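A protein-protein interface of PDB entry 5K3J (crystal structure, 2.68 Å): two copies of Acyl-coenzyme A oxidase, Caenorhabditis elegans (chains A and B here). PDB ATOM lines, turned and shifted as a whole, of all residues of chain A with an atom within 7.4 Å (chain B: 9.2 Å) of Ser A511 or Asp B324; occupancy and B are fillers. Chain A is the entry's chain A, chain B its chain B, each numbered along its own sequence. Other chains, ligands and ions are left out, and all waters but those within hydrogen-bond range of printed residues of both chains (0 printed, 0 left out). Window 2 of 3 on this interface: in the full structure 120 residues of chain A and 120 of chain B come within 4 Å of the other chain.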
ATOM      1  N   PHE A 502     -15.887  19.746   0.925  1.00  0.00           N
ATOM      2  CA  PHE A 502     -14.477  19.379   0.886  1.00  0.00           C
ATOM      3  C   PHE A 502     -13.875  19.445   2.291  1.00  0.00           C
ATOM      4  O   PHE A 502     -13.082  18.584   2.666  1.00  0.00           O
ATOM      5  CB  PHE A 502     -13.715  20.282  -0.090  1.00  0.00           C
ATOM      6  CG  PHE A 502     -12.232  20.329   0.142  1.00  0.00           C
ATOM      7  CD1 PHE A 502     -11.457  19.181   0.079  1.00  0.00           C
ATOM      8  CD2 PHE A 502     -11.607  21.538   0.389  1.00  0.00           C
ATOM      9  CE1 PHE A 502     -10.089  19.242   0.287  1.00  0.00           C
ATOM     10  CE2 PHE A 502     -10.245  21.602   0.593  1.00  0.00           C
ATOM     11  CZ  PHE A 502      -9.486  20.453   0.542  1.00  0.00           C
ATOM     12  N   LEU A 505     -15.008  16.454   4.528  1.00  0.00           N
ATOM     13  CA  LEU A 505     -14.306  15.231   4.164  1.00  0.00           C
ATOM     14  C   LEU A 505     -12.920  15.172   4.799  1.00  0.00           C
ATOM     15  O   LEU A 505     -12.314  14.107   4.877  1.00  0.00           O
ATOM     16  CB  LEU A 505     -14.202  15.108   2.641  1.00  0.00           C
ATOM     17  CG  LEU A 505     -15.507  14.774   1.910  1.00  0.00           C
ATOM     18  CD1 LEU A 505     -15.472  15.284   0.479  1.00  0.00           C
ATOM     19  CD2 LEU A 505     -15.771  13.272   1.935  1.00  0.00           C
ATOM     20  N   MET A 506     -12.417  16.313   5.257  1.00  0.00           N
ATOM     21  CA  MET A 506     -11.133  16.338   5.953  1.00  0.00           C
ATOM     22  C   MET A 506     -11.348  16.215   7.457  1.00  0.00           C
ATOM     23  O   MET A 506     -10.483  15.722   8.182  1.00  0.00           O
ATOM     24  CB  MET A 506     -10.356  17.612   5.622  1.00  0.00           C
ATOM     25  CG  MET A 506     -10.091  17.793   4.136  1.00  0.00           C
ATOM     26  SD  MET A 506      -8.920  19.118   3.793  1.00  0.00           S
ATOM     27  CE  MET A 506      -7.417  18.423   4.470  1.00  0.00           C
ATOM     28  N   SER A 508     -13.570  14.330   8.244  1.00  0.00           N
ATOM     29  CA  SER A 508     -13.759  12.887   8.174  1.00  0.00           C
ATOM     30  C   SER A 508     -12.398  12.207   8.255  1.00  0.00           C
ATOM     31  O   SER A 508     -12.299  11.007   8.499  1.00  0.00           O
ATOM     32  CB  SER A 508     -14.482  12.483   6.886  1.00  0.00           C
ATOM     33  OG  SER A 508     -15.810  12.976   6.859  1.00  0.00           O
ATOM     34  N   GLY A 509     -11.342  12.984   8.049  1.00  0.00           N
ATOM     35  CA  GLY A 509      -9.995  12.455   8.105  1.00  0.00           C
ATOM     36  C   GLY A 509      -9.567  11.820   6.797  1.00  0.00           C
ATOM     37  O   GLY A 509      -8.580  11.088   6.749  1.00  0.00           O
ATOM     38  N   GLU A 510     -10.320  12.083   5.736  1.00  0.00           N
ATOM     39  CA  GLU A 510      -9.900  11.676   4.403  1.00  0.00           C
ATOM     40  C   GLU A 510      -8.847  12.674   3.943  1.00  0.00           C
ATOM     41  O   GLU A 510      -9.035  13.883   4.083  1.00  0.00           O
ATOM     42  CB  GLU A 510     -11.086  11.626   3.434  1.00  0.00           C
ATOM     43  CG  GLU A 510     -11.040  10.489   2.422  1.00  0.00           C
ATOM     44  CD  GLU A 510     -11.580   9.180   2.975  1.00  0.00           C
ATOM     45  OE1 GLU A 510     -11.714   9.055   4.211  1.00  0.00           O
ATOM     46  OE2 GLU A 510     -11.878   8.273   2.169  1.00  0.00           O
ATOM     47  N   SER A 511      -7.738  12.162   3.416  1.00  0.00           N
ATOM     48  CA  SER A 511      -6.600  13.001   3.045  1.00  0.00           C
ATOM     49  C   SER A 511      -7.000  14.081   2.048  1.00  0.00           C
ATOM     50  O   SER A 511      -7.950  13.907   1.287  1.00  0.00           O
ATOM     51  CB  SER A 511      -5.471  12.151   2.463  1.00  0.00           C
ATOM     52  OG  SER A 511      -5.568  12.068   1.051  1.00  0.00           O
ATOM     53  N   ARG A 512      -6.261  15.187   2.061  1.00  0.00           N
ATOM     54  CA  ARG A 512      -6.581  16.361   1.249  1.00  0.00           C
ATOM     55  C   ARG A 512      -6.814  16.033  -0.220  1.00  0.00           C
ATOM     56  O   ARG A 512      -7.852  16.383  -0.782  1.00  0.00           O
ATOM     57  CB  ARG A 512      -5.466  17.400   1.352  1.00  0.00           C
ATOM     58  CG  ARG A 512      -5.622  18.541   0.363  1.00  0.00           C
ATOM     59  CD  ARG A 512      -4.520  19.568   0.506  1.00  0.00           C
ATOM     60  NE  ARG A 512      -4.970  20.881   0.054  1.00  0.00           N
ATOM     61  CZ  ARG A 512      -5.490  21.806   0.856  1.00  0.00           C
ATOM     62  NH1 ARG A 512      -5.878  22.972   0.359  1.00  0.00           N
ATOM     63  NH2 ARG A 512      -5.620  21.566   2.156  1.00  0.00           N
ATOM     64  N   GLU A 513      -5.839  15.368  -0.831  1.00  0.00           N
ATOM     65  CA  GLU A 513      -5.925  14.977  -2.233  1.00  0.00           C
ATOM     66  C   GLU A 513      -7.208  14.206  -2.536  1.00  0.00           C
ATOM     67  O   GLU A 513      -7.894  14.486  -3.518  1.00  0.00           O
ATOM     68  CB  GLU A 513      -4.706  14.137  -2.623  1.00  0.00           C
ATOM     69  CG  GLU A 513      -3.444  14.940  -2.920  1.00  0.00           C
ATOM     70  CD  GLU A 513      -2.821  15.558  -1.680  1.00  0.00           C
ATOM     71  OE1 GLU A 513      -3.072  15.049  -0.566  1.00  0.00           O
ATOM     72  OE2 GLU A 513      -2.081  16.555  -1.821  1.00  0.00           O
ATOM     73  N   VAL A 514      -7.531  13.237  -1.687  1.00  0.00           N
ATOM     74  CA  VAL A 514      -8.730  12.432  -1.881  1.00  0.00           C
ATOM     75  C   VAL A 514      -9.981  13.228  -1.522  1.00  0.00           C
ATOM     76  O   VAL A 514     -11.005  13.131  -2.202  1.00  0.00           O
ATOM     77  CB  VAL A 514      -8.676  11.132  -1.047  1.00  0.00           C
ATOM     78  CG1 VAL A 514      -9.971  10.341  -1.187  1.00  0.00           C
ATOM     79  CG2 VAL A 514      -7.489  10.286  -1.472  1.00  0.00           C
ATOM     80  N   ALA A 515      -9.894  14.015  -0.455  1.00  0.00           N
ATOM     81  CA  ALA A 515     -10.981  14.908  -0.075  1.00  0.00           C
ATOM     82  C   ALA A 515     -11.275  15.897  -1.195  1.00  0.00           C
ATOM     83  O   ALA A 515     -12.430  16.196  -1.488  1.00  0.00           O
ATOM     84  CB  ALA A 515     -10.638  15.645   1.205  1.00  0.00           C
ATOM     85  N   TRP A 516     -10.215  16.402  -1.817  1.00  0.00           N
ATOM     86  CA  TRP A 516     -10.347  17.291  -2.965  1.00  0.00           C
ATOM     87  C   TRP A 516     -10.997  16.569  -4.140  1.00  0.00           C
ATOM     88  O   TRP A 516     -11.872  17.114  -4.816  1.00  0.00           O
ATOM     89  CB  TRP A 516      -8.982  17.842  -3.387  1.00  0.00           C
ATOM     90  CG  TRP A 516      -9.067  18.746  -4.567  1.00  0.00           C
ATOM     91  CD1 TRP A 516      -8.789  18.430  -5.865  1.00  0.00           C
ATOM     92  CD2 TRP A 516      -9.478  20.116  -4.566  1.00  0.00           C
ATOM     93  NE1 TRP A 516      -8.995  19.521  -6.673  1.00  0.00           N
ATOM     94  CE2 TRP A 516      -9.418  20.568  -5.900  1.00  0.00           C
ATOM     95  CE3 TRP A 516      -9.885  21.004  -3.569  1.00  0.00           C
ATOM     96  CZ2 TRP A 516      -9.750  21.867  -6.260  1.00  0.00           C
ATOM     97  CZ3 TRP A 516     -10.213  22.294  -3.929  1.00  0.00           C
ATOM     98  CH2 TRP A 516     -10.148  22.713  -5.263  1.00  0.00           C
ATOM     99  N   ASN A 517     -10.557  15.337  -4.372  1.00  0.00           N
ATOM    100  CA  ASN A 517     -11.012  14.539  -5.502  1.00  0.00           C
ATOM    101  C   ASN A 517     -12.506  14.228  -5.429  1.00  0.00           C
ATOM    102  O   ASN A 517     -13.218  14.327  -6.428  1.00  0.00           O
ATOM    103  CB  ASN A 517     -10.207  13.239  -5.573  1.00  0.00           C
ATOM    104  CG  ASN A 517     -10.485  12.439  -6.832  1.00  0.00           C
ATOM    105  OD1 ASN A 517     -11.205  12.884  -7.724  1.00  0.00           O
ATOM    106  ND2 ASN A 517      -9.900  11.250  -6.913  1.00  0.00           N
ATOM    107  N   GLY B 321      -0.876  13.436 -12.993  1.00  0.00           N
ATOM    108  CA  GLY B 321      -1.174  14.009 -11.694  1.00  0.00           C
ATOM    109  C   GLY B 321      -1.185  12.964 -10.598  1.00  0.00           C
ATOM    110  O   GLY B 321      -1.371  11.774 -10.860  1.00  0.00           O
ATOM    111  N   HIS B 322      -0.981  13.413  -9.363  1.00  0.00           N
ATOM    112  CA  HIS B 322      -0.978  12.524  -8.201  1.00  0.00           C
ATOM    113  C   HIS B 322      -2.192  12.753  -7.300  1.00  0.00           C
ATOM    114  O   HIS B 322      -2.729  13.861  -7.233  1.00  0.00           O
ATOM    115  CB  HIS B 322       0.301  12.715  -7.374  1.00  0.00           C
ATOM    116  CG  HIS B 322       1.565  12.645  -8.174  1.00  0.00           C
ATOM    117  ND1 HIS B 322       2.391  11.540  -8.172  1.00  0.00           N
ATOM    118  CD2 HIS B 322       2.153  13.549  -8.992  1.00  0.00           C
ATOM    119  CE1 HIS B 322       3.427  11.764  -8.960  1.00  0.00           C
ATOM    120  NE2 HIS B 322       3.306  12.977  -9.471  1.00  0.00           N
ATOM    121  N   LEU B 323      -2.626  11.698  -6.617  1.00  0.00           N
ATOM    122  CA  LEU B 323      -3.572  11.822  -5.512  1.00  0.00           C
ATOM    123  C   LEU B 323      -2.777  11.632  -4.231  1.00  0.00           C
ATOM    124  O   LEU B 323      -1.830  12.373  -3.959  1.00  0.00           O
ATOM    125  CB  LEU B 323      -4.687  10.781  -5.599  1.00  0.00           C
ATOM    126  CG  LEU B 323      -5.692  10.872  -6.741  1.00  0.00           C
ATOM    127  CD1 LEU B 323      -6.668   9.705  -6.673  1.00  0.00           C
ATOM    128  CD2 LEU B 323      -6.435  12.199  -6.700  1.00  0.00           C
ATOM    129  N   ASP B 324      -3.162  10.625  -3.454  1.00  0.00           N
ATOM    130  CA  ASP B 324      -2.253  10.030  -2.489  1.00  0.00           C
ATOM    131  C   ASP B 324      -1.160   9.352  -3.310  1.00  0.00           C
ATOM    132  O   ASP B 324      -1.308   9.217  -4.527  1.00  0.00           O
ATOM    133  CB  ASP B 324      -2.974   9.032  -1.580  1.00  0.00           C
ATOM    134  CG  ASP B 324      -3.886   9.711  -0.570  1.00  0.00           C
ATOM    135  OD1 ASP B 324      -4.200  10.904  -0.758  1.00  0.00           O
ATOM    136  OD2 ASP B 324      -4.288   9.051   0.412  1.00  0.00           O
ATOM    137  N   ASP B 325      -0.074   8.937  -2.661  1.00  0.00           N
ATOM    138  CA  ASP B 325       1.042   8.282  -3.348  1.00  0.00           C
ATOM    139  C   ASP B 325       1.700   9.250  -4.334  1.00  0.00           C
ATOM    140  O   ASP B 325       1.259   9.386  -5.476  1.00  0.00           O
ATOM    141  CB  ASP B 325       0.563   7.009  -4.065  1.00  0.00           C
ATOM    142  CG  ASP B 325       1.702   6.165  -4.614  1.00  0.00           C
ATOM    143  OD1 ASP B 325       2.858   6.639  -4.645  1.00  0.00           O
ATOM    144  OD2 ASP B 325       1.430   5.018  -5.025  1.00  0.00           O
ATOM    145  N   LYS B 326       2.761   9.916  -3.886  1.00  0.00           N
ATOM    146  CA  LYS B 326       3.459  10.902  -4.709  1.00  0.00           C
ATOM    147  C   LYS B 326       4.658  10.317  -5.450  1.00  0.00           C
ATOM    148  O   LYS B 326       5.575  11.044  -5.830  1.00  0.00           O
ATOM    149  CB  LYS B 326       3.919  12.077  -3.845  1.00  0.00           C
ATOM    150  CG  LYS B 326       2.843  13.113  -3.572  1.00  0.00           C
ATOM    151  CD  LYS B 326       2.531  13.954  -4.809  1.00  0.00           C
ATOM    152  CE  LYS B 326       3.658  14.929  -5.163  1.00  0.00           C
ATOM    153  NZ  LYS B 326       4.738  14.325  -5.998  1.00  0.00           N
ATOM    154  N   GLN B 327       4.649   9.004  -5.651  1.00  0.00           N
ATOM    155  CA  GLN B 327       5.730   8.339  -6.364  1.00  0.00           C
ATOM    156  C   GLN B 327       5.252   7.887  -7.734  1.00  0.00           C
ATOM    157  O   GLN B 327       6.031   7.824  -8.686  1.00  0.00           O
ATOM    158  CB  GLN B 327       6.253   7.147  -5.562  1.00  0.00           C
ATOM    159  CG  GLN B 327       7.503   6.493  -6.138  1.00  0.00           C
ATOM    160  CD  GLN B 327       8.755   7.330  -5.938  1.00  0.00           C
ATOM    161  OE1 GLN B 327       8.812   8.190  -5.056  1.00  0.00           O
ATOM    162  NE2 GLN B 327       9.769   7.077  -6.757  1.00  0.00           N
ATOM    163  N   VAL B 328       3.966   7.565  -7.824  1.00  0.00           N
ATOM    164  CA  VAL B 328       3.363   7.151  -9.085  1.00  0.00           C
ATOM    165  C   VAL B 328       2.104   7.961  -9.359  1.00  0.00           C
ATOM    166  O   VAL B 328       1.212   8.040  -8.513  1.00  0.00           O
ATOM    167  CB  VAL B 328       3.007   5.653  -9.087  1.00  0.00           C
ATOM    168  CG1 VAL B 328       2.315   5.269 -10.392  1.00  0.00           C
ATOM    169  CG2 VAL B 328       4.259   4.805  -8.860  1.00  0.00           C
ATOM    170  N   GLU B 329       2.040   8.565 -10.540  1.00  0.00           N
ATOM    171  CA  GLU B 329       0.859   9.311 -10.948  1.00  0.00           C
ATOM    172  C   GLU B 329      -0.314   8.358 -11.142  1.00  0.00           C
ATOM    173  O   GLU B 329      -0.120   7.170 -11.404  1.00  0.00           O
ATOM    174  CB  GLU B 329       1.133  10.098 -12.232  1.00  0.00           C
ATOM    175  CG  GLU B 329       2.482  10.802 -12.244  1.00  0.00           C
ATOM    176  CD  GLU B 329       2.617  11.800 -13.375  1.00  0.00           C
ATOM    177  OE1 GLU B 329       3.691  11.839 -14.010  1.00  0.00           O
ATOM    178  OE2 GLU B 329       1.648  12.546 -13.626  1.00  0.00           O
ATOM    179  N   VAL B 330      -1.529   8.879 -11.010  1.00  0.00           N
ATOM    180  CA  VAL B 330      -2.725   8.048 -11.073  1.00  0.00           C
ATOM    181  C   VAL B 330      -3.320   7.996 -12.474  1.00  0.00           C
ATOM    182  O   VAL B 330      -3.217   8.959 -13.238  1.00  0.00           O
ATOM    183  CB  VAL B 330      -3.813   8.555 -10.101  1.00  0.00           C
ATOM    184  CG1 VAL B 330      -3.344   8.448  -8.656  1.00  0.00           C
ATOM    185  CG2 VAL B 330      -4.194   9.985 -10.438  1.00  0.00           C
ATOM    186  N   LYS B 331      -3.936   6.863 -12.808  1.00  0.00           N
ATOM    187  CA  LYS B 331      -4.745   6.767 -14.017  1.00  0.00           C
ATOM    188  C   LYS B 331      -5.811   7.852 -13.967  1.00  0.00           C
ATOM    189  O   LYS B 331      -6.449   8.054 -12.933  1.00  0.00           O
ATOM    190  CB  LYS B 331      -5.394   5.390 -14.143  1.00  0.00           C
ATOM    191  CG  LYS B 331      -4.403   4.245 -14.261  1.00  0.00           C
ATOM    192  CD  LYS B 331      -5.113   2.913 -14.409  1.00  0.00           C
ATOM    193  CE  LYS B 331      -4.120   1.780 -14.595  1.00  0.00           C
ATOM    194  NZ  LYS B 331      -4.805   0.497 -14.910  1.00  0.00           N
ATOM    195  N   ASP B 334      -9.288   7.691 -12.511  1.00  0.00           N
ATOM    196  CA  ASP B 334      -9.463   7.715 -11.061  1.00  0.00           C
ATOM    197  C   ASP B 334      -9.992   9.068 -10.574  1.00  0.00           C
ATOM    198  O   ASP B 334     -10.430   9.200  -9.428  1.00  0.00           O
ATOM    199  CB  ASP B 334      -8.142   7.390 -10.357  1.00  0.00           C
ATOM    200  CG  ASP B 334      -7.835   5.899 -10.344  1.00  0.00           C
ATOM    201  OD1 ASP B 334      -8.777   5.096 -10.525  1.00  0.00           O
ATOM    202  OD2 ASP B 334      -6.660   5.526 -10.138  1.00  0.00           O
ATOM    203  N   TYR B 335      -9.950  10.072 -11.446  1.00  0.00           N
ATOM    204  CA  TYR B 335     -10.439  11.406 -11.104  1.00  0.00           C
ATOM    205  C   TYR B 335     -11.958  11.488 -11.238  1.00  0.00           C
ATOM    206  O   TYR B 335     -12.536  10.901 -12.150  1.00  0.00           O
ATOM    207  CB  TYR B 335      -9.775  12.460 -11.992  1.00  0.00           C
ATOM    208  CG  TYR B 335      -8.301  12.659 -11.727  1.00  0.00           C
ATOM    209  CD1 TYR B 335      -7.829  12.894 -10.440  1.00  0.00           C
ATOM    210  CD2 TYR B 335      -7.379  12.611 -12.762  1.00  0.00           C
ATOM    211  CE1 TYR B 335      -6.484  13.076 -10.195  1.00  0.00           C
ATOM    212  CE2 TYR B 335      -6.031  12.791 -12.522  1.00  0.00           C
ATOM    213  CZ  TYR B 335      -5.590  13.025 -11.239  1.00  0.00           C
ATOM    214  OH  TYR B 335      -4.248  13.205 -10.992  1.00  0.00           O
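Along chain B the printed residues that touch a printed residue of chain A span positions 323 to 335.
Among the printed residues, 7 pairs touch across the chains.
The side-chain hydroxyl (OH) of Tyr B335 sits close to the backbone carbonyl oxygen (O) of Gly B321, at 3.2 Å.
No position is printed for both chains.
Among the printed residues, merely in contact across the chains: Glu A513 with Leu B323 (3.2 Å), Glu A513 with Asp B324 (3.8 Å), Val A514 with Asp B324 (3.4 Å), Asn A517 with Leu B323 (3.6 Å) and Asn A517 with Tyr B335 (3.8 Å).
OG of Ser A511 is in hydrogen-bond range of OD1 of Asp B324 (2.5 Å).
The backbone carbonyl oxygen (O) of Asp B334 is in hydrogen-bond range of the side-chain amide nitrogen (ND2) of Asn A517.
Gly A509 touches none of the printed residues of chain B.
Of chain B, only Asp B324 comes within 4 Å of Ser A511.
Of chain B, only Asp B324 (3.4 Å) comes within 4 Å of Val A514.
Asp B324 touches just these residues of chain A: Ser A511 (2.5 Å), Glu A513 (3.8 Å) and Val A514 (3.4 Å).
Val B330 touches none of the printed residues of chain A.
Of the printed residues of chain A, Asp B334 touches Asn A517.
Of the printed residues of chain A, Tyr B335 touches Asn A517.
The nearest residue of chain A that does not touch Asp B324 is Arg A512 (5.5 Å).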
